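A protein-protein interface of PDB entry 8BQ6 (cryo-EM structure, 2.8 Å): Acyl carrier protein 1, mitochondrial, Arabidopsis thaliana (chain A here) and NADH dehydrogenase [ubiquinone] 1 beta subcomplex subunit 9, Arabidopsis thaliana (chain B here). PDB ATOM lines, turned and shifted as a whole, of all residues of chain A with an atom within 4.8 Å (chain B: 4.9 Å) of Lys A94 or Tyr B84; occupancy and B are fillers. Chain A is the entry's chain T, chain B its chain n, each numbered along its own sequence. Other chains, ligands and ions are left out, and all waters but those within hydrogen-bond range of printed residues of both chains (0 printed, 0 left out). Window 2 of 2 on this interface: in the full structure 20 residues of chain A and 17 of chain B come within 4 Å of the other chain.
The backbone NH (N) of Val B86 lies within hydrogen-bond range of the side-chain carboxylate (OE1) of Glu A96.
Of the 8 printed residues of chain A, 4 touch a printed residue of chain B.
Hydrophobic or aromatic side chains of chain A that line the printed part of chain B: Leu A95 and Met A120.
Hydrophobic or aromatic side chains of chain B that line the printed part of chain A: Tyr B84, Ile B85, Val B86 and Trp B88.
Among the printed residues, 7 pairs touch across the chains.
Among the printed residues, no Asp or Glu carboxylate lies within 4 Å of a Lys or Arg side-chain nitrogen of the other chain.
O of Glu A90 is in hydrogen-bond range of N of Leu A95 (3.0 Å).
The backbone NH of Tyr B84 sits at hydrogen-bond distance from the side-chain amide oxygen of Asn B33 (3.0 Å).
Of chain B, only Tyr B84 (3.8 Å) and Trp B88 (3.3 Å) come within 4 Å of Lys A94.
Of chain A, only Lys A94 comes within 4 Å of Tyr B84.
Of the printed residues of chain A, Val B86 touches Glu A96 (3.0 Å).
Printed residues of chain A within 4 Å of Ile B85: Glu A96.
Pro B87 touches none of the printed residues of chain A.
The nearest printed residue of chain B that does not touch Met A120 is Val B86 (6.9 Å).
Among the printed residues, merely in contact across the chains: Lys A94 with Tyr B84 (3.8 Å), Lys A94 with Trp B88 (3.3 Å), Leu A95 with Trp B88 (3.7 Å), Glu A96 with Ile B85 (3.7 Å), Glu A96 with Trp B88 (3.7 Å) and Met A120 with Trp B88 (3.2 Å).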
ATOM      1  N   GLU A  90     -23.228  -3.901  25.885  1.00  0.00           N
ATOM      2  CA  GLU A  90     -22.138  -4.420  25.067  1.00  0.00           C
ATOM      3  C   GLU A  90     -21.864  -5.885  25.358  1.00  0.00           C
ATOM      4  O   GLU A  90     -21.795  -6.709  24.440  1.00  0.00           O
ATOM      5  CB  GLU A  90     -20.880  -3.594  25.300  1.00  0.00           C
ATOM      6  CG  GLU A  90     -20.485  -2.819  24.093  1.00  0.00           C
ATOM      7  CD  GLU A  90     -19.516  -1.718  24.395  1.00  0.00           C
ATOM      8  OE1 GLU A  90     -19.647  -0.647  23.770  1.00  0.00           O
ATOM      9  OE2 GLU A  90     -18.623  -1.917  25.241  1.00  0.00           O
ATOM     10  N   GLU A  91     -21.703  -6.229  26.634  1.00  0.00           N
ATOM     11  CA  GLU A  91     -21.428  -7.608  27.007  1.00  0.00           C
ATOM     12  C   GLU A  91     -22.618  -8.521  26.758  1.00  0.00           C
ATOM     13  O   GLU A  91     -22.439  -9.731  26.586  1.00  0.00           O
ATOM     14  CB  GLU A  91     -21.026  -7.677  28.476  1.00  0.00           C
ATOM     15  CG  GLU A  91     -20.253  -8.915  28.837  1.00  0.00           C
ATOM     16  CD  GLU A  91     -19.218  -8.649  29.903  1.00  0.00           C
ATOM     17  OE1 GLU A  91     -18.450  -9.577  30.231  1.00  0.00           O
ATOM     18  OE2 GLU A  91     -19.172  -7.509  30.413  1.00  0.00           O
ATOM     19  N   GLU A  92     -23.832  -7.971  26.749  1.00  0.00           N
ATOM     20  CA  GLU A  92     -25.005  -8.820  26.595  1.00  0.00           C
ATOM     21  C   GLU A  92     -25.100  -9.388  25.187  1.00  0.00           C
ATOM     22  O   GLU A  92     -25.455 -10.560  25.013  1.00  0.00           O
ATOM     23  CB  GLU A  92     -26.271  -8.038  26.941  1.00  0.00           C
ATOM     24  CG  GLU A  92     -27.548  -8.774  26.592  1.00  0.00           C
ATOM     25  CD  GLU A  92     -27.798  -9.940  27.530  1.00  0.00           C
ATOM     26  OE1 GLU A  92     -27.141  -9.997  28.587  1.00  0.00           O
ATOM     27  OE2 GLU A  92     -28.648 -10.799  27.216  1.00  0.00           O
ATOM     28  N   PHE A  93     -24.788  -8.578  24.180  1.00  0.00           N
ATOM     29  CA  PHE A  93     -24.800  -9.000  22.789  1.00  0.00           C
ATOM     30  C   PHE A  93     -23.400  -9.205  22.231  1.00  0.00           C
ATOM     31  O   PHE A  93     -23.257  -9.440  21.027  1.00  0.00           O
ATOM     32  CB  PHE A  93     -25.552  -7.973  21.936  1.00  0.00           C
ATOM     33  CG  PHE A  93     -27.000  -7.822  22.303  1.00  0.00           C
ATOM     34  CD1 PHE A  93     -27.943  -8.717  21.836  1.00  0.00           C
ATOM     35  CD2 PHE A  93     -27.421  -6.776  23.106  1.00  0.00           C
ATOM     36  CE1 PHE A  93     -29.272  -8.578  22.167  1.00  0.00           C
ATOM     37  CE2 PHE A  93     -28.750  -6.637  23.440  1.00  0.00           C
ATOM     38  CZ  PHE A  93     -29.674  -7.539  22.970  1.00  0.00           C
ATOM     39  N   LYS A  94     -22.371  -9.117  23.077  1.00  0.00           N
ATOM     40  CA  LYS A  94     -20.970  -9.259  22.679  1.00  0.00           C
ATOM     41  C   LYS A  94     -20.646  -8.393  21.461  1.00  0.00           C
ATOM     42  O   LYS A  94     -20.297  -8.883  20.386  1.00  0.00           O
ATOM     43  CB  LYS A  94     -20.617 -10.724  22.418  1.00  0.00           C
ATOM     44  CG  LYS A  94     -19.131 -11.000  22.450  1.00  0.00           C
ATOM     45  CD  LYS A  94     -18.824 -12.317  21.784  1.00  0.00           C
ATOM     46  CE  LYS A  94     -17.334 -12.558  21.687  1.00  0.00           C
ATOM     47  NZ  LYS A  94     -17.072 -13.846  20.996  1.00  0.00           N
ATOM     48  N   LEU A  95     -20.787  -7.085  21.681  1.00  0.00           N
ATOM     49  CA  LEU A  95     -20.486  -6.118  20.604  1.00  0.00           C
ATOM     50  C   LEU A  95     -19.353  -5.199  21.052  1.00  0.00           C
ATOM     51  O   LEU A  95     -19.116  -5.093  22.271  1.00  0.00           O
ATOM     52  CB  LEU A  95     -21.736  -5.277  20.321  1.00  0.00           C
ATOM     53  CG  LEU A  95     -22.967  -6.027  19.823  1.00  0.00           C
ATOM     54  CD1 LEU A  95     -24.154  -5.085  19.703  1.00  0.00           C
ATOM     55  CD2 LEU A  95     -22.689  -6.699  18.490  1.00  0.00           C
ATOM     56  N   GLU A  96     -18.653  -4.600  20.100  1.00  0.00           N
ATOM     57  CA  GLU A  96     -17.625  -3.602  20.378  1.00  0.00           C
ATOM     58  C   GLU A  96     -18.064  -2.309  19.700  1.00  0.00           C
ATOM     59  O   GLU A  96     -17.735  -2.058  18.539  1.00  0.00           O
ATOM     60  CB  GLU A  96     -16.241  -4.048  19.900  1.00  0.00           C
ATOM     61  CG  GLU A  96     -15.125  -3.144  20.405  1.00  0.00           C
ATOM     62  CD  GLU A  96     -13.825  -3.878  20.702  1.00  0.00           C
ATOM     63  OE1 GLU A  96     -13.863  -4.980  21.288  1.00  0.00           O
ATOM     64  OE2 GLU A  96     -12.754  -3.333  20.365  1.00  0.00           O
ATOM     65  N   MET A 120     -24.049  -8.686  14.146  1.00  0.00           N
ATOM     66  CA  MET A 120     -23.162  -9.605  14.913  1.00  0.00           C
ATOM     67  C   MET A 120     -23.648  -9.716  16.364  1.00  0.00           C
ATOM     68  O   MET A 120     -22.862 -10.192  17.212  1.00  0.00           O
ATOM     69  CB  MET A 120     -21.715  -9.099  14.904  1.00  0.00           C
ATOM     70  CG  MET A 120     -21.060  -9.113  13.538  1.00  0.00           C
ATOM     71  SD  MET A 120     -20.992 -10.773  12.825  1.00  0.00           S
ATOM     72  CE  MET A 120     -19.846 -11.564  13.953  1.00  0.00           C
ATOM     73  N   ASN B  33      -9.468  -5.510  31.712  1.00  0.00           N
ATOM     74  CA  ASN B  33      -8.279  -6.129  31.131  1.00  0.00           C
ATOM     75  C   ASN B  33      -7.265  -6.499  32.201  1.00  0.00           C
ATOM     76  O   ASN B  33      -6.612  -7.545  32.115  1.00  0.00           O
ATOM     77  CB  ASN B  33      -7.630  -5.197  30.111  1.00  0.00           C
ATOM     78  CG  ASN B  33      -8.352  -5.187  28.792  1.00  0.00           C
ATOM     79  OD1 ASN B  33      -8.791  -6.227  28.308  1.00  0.00           O
ATOM     80  ND2 ASN B  33      -8.475  -4.009  28.196  1.00  0.00           N
ATOM     81  N   ASP B  82      -2.015  -5.223  26.396  1.00  0.00           N
ATOM     82  CA  ASP B  82      -2.714  -6.196  25.555  1.00  0.00           C
ATOM     83  C   ASP B  82      -4.201  -6.146  25.866  1.00  0.00           C
ATOM     84  O   ASP B  82      -4.724  -6.999  26.597  1.00  0.00           O
ATOM     85  CB  ASP B  82      -2.159  -7.605  25.758  1.00  0.00           C
ATOM     86  CG  ASP B  82      -2.326  -8.472  24.534  1.00  0.00           C
ATOM     87  OD1 ASP B  82      -2.556  -9.688  24.694  1.00  0.00           O
ATOM     88  OD2 ASP B  82      -2.234  -7.933  23.410  1.00  0.00           O
ATOM     89  N   PRO B  83      -4.915  -5.159  25.334  1.00  0.00           N
ATOM     90  CA  PRO B  83      -6.353  -5.071  25.594  1.00  0.00           C
ATOM     91  C   PRO B  83      -7.132  -6.147  24.858  1.00  0.00           C
ATOM     92  O   PRO B  83      -6.685  -6.703  23.852  1.00  0.00           O
ATOM     93  CB  PRO B  83      -6.720  -3.677  25.079  1.00  0.00           C
ATOM     94  CG  PRO B  83      -5.707  -3.394  24.044  1.00  0.00           C
ATOM     95  CD  PRO B  83      -4.433  -4.026  24.525  1.00  0.00           C
ATOM     96  N   TYR B  84      -8.318  -6.436  25.382  1.00  0.00           N
ATOM     97  CA  TYR B  84      -9.192  -7.407  24.750  1.00  0.00           C
ATOM     98  C   TYR B  84      -9.917  -6.774  23.572  1.00  0.00           C
ATOM     99  O   TYR B  84     -10.331  -5.613  23.627  1.00  0.00           O
ATOM    100  CB  TYR B  84     -10.209  -7.940  25.753  1.00  0.00           C
ATOM    101  CG  TYR B  84     -11.278  -8.757  25.091  1.00  0.00           C
ATOM    102  CD1 TYR B  84     -11.021 -10.051  24.675  1.00  0.00           C
ATOM    103  CD2 TYR B  84     -12.529  -8.220  24.834  1.00  0.00           C
ATOM    104  CE1 TYR B  84     -11.985 -10.796  24.048  1.00  0.00           C
ATOM    105  CE2 TYR B  84     -13.497  -8.957  24.207  1.00  0.00           C
ATOM    106  CZ  TYR B  84     -13.221 -10.247  23.820  1.00  0.00           C
ATOM    107  OH  TYR B  84     -14.185 -10.993  23.191  1.00  0.00           O
ATOM    108  N   ILE B  85     -10.072  -7.541  22.498  1.00  0.00           N
ATOM    109  CA  ILE B  85     -10.795  -7.090  21.317  1.00  0.00           C
ATOM    110  C   ILE B  85     -11.754  -8.189  20.897  1.00  0.00           C
ATOM    111  O   ILE B  85     -11.368  -9.362  20.828  1.00  0.00           O
ATOM    112  CB  ILE B  85      -9.842  -6.738  20.160  1.00  0.00           C
ATOM    113  CG1 ILE B  85      -8.793  -5.736  20.633  1.00  0.00           C
ATOM    114  CG2 ILE B  85     -10.616  -6.150  18.996  1.00  0.00           C
ATOM    115  CD1 ILE B  85      -7.416  -6.037  20.133  1.00  0.00           C
ATOM    116  N   VAL B  86     -12.999  -7.814  20.629  1.00  0.00           N
ATOM    117  CA  VAL B  86     -13.922  -8.760  19.999  1.00  0.00           C
ATOM    118  C   VAL B  86     -13.317  -9.205  18.674  1.00  0.00           C
ATOM    119  O   VAL B  86     -12.826  -8.355  17.906  1.00  0.00           O
ATOM    120  CB  VAL B  86     -15.298  -8.107  19.788  1.00  0.00           C
ATOM    121  CG1 VAL B  86     -16.302  -9.130  19.329  1.00  0.00           C
ATOM    122  CG2 VAL B  86     -15.770  -7.434  21.062  1.00  0.00           C
ATOM    123  N   PRO B  87     -13.292 -10.503  18.364  1.00  0.00           N
ATOM    124  CA  PRO B  87     -12.513 -10.963  17.202  1.00  0.00           C
ATOM    125  C   PRO B  87     -12.907 -10.328  15.878  1.00  0.00           C
ATOM    126  O   PRO B  87     -12.023 -10.069  15.053  1.00  0.00           O
ATOM    127  CB  PRO B  87     -12.756 -12.476  17.202  1.00  0.00           C
ATOM    128  CG  PRO B  87     -13.012 -12.798  18.631  1.00  0.00           C
ATOM    129  CD  PRO B  87     -13.762 -11.629  19.191  1.00  0.00           C
ATOM    130  N   TRP B  88     -14.201 -10.050  15.683  1.00  0.00           N
ATOM    131  CA  TRP B  88     -14.676  -9.463  14.396  1.00  0.00           C
ATOM    132  C   TRP B  88     -14.479  -7.941  14.377  1.00  0.00           C
ATOM    133  O   TRP B  88     -14.630  -7.356  13.289  1.00  0.00           O
ATOM    134  CB  TRP B  88     -16.136  -9.848  14.097  1.00  0.00           C
ATOM    135  CG  TRP B  88     -17.108  -9.661  15.223  1.00  0.00           C
ATOM    136  CD1 TRP B  88     -17.639 -10.642  16.008  1.00  0.00           C
ATOM    137  CD2 TRP B  88     -17.706  -8.428  15.665  1.00  0.00           C
ATOM    138  NE1 TRP B  88     -18.511 -10.107  16.917  1.00  0.00           N
ATOM    139  CE2 TRP B  88     -18.572  -8.752  16.732  1.00  0.00           C
ATOM    140  CE3 TRP B  88     -17.600  -7.088  15.276  1.00  0.00           C
ATOM    141  CZ2 TRP B  88     -19.308  -7.784  17.410  1.00  0.00           C
ATOM    142  CZ3 TRP B  88     -18.324  -6.132  15.949  1.00  0.00           C
ATOM    143  CH2 TRP B  88     -19.169  -6.478  17.002  1.00  0.00           C
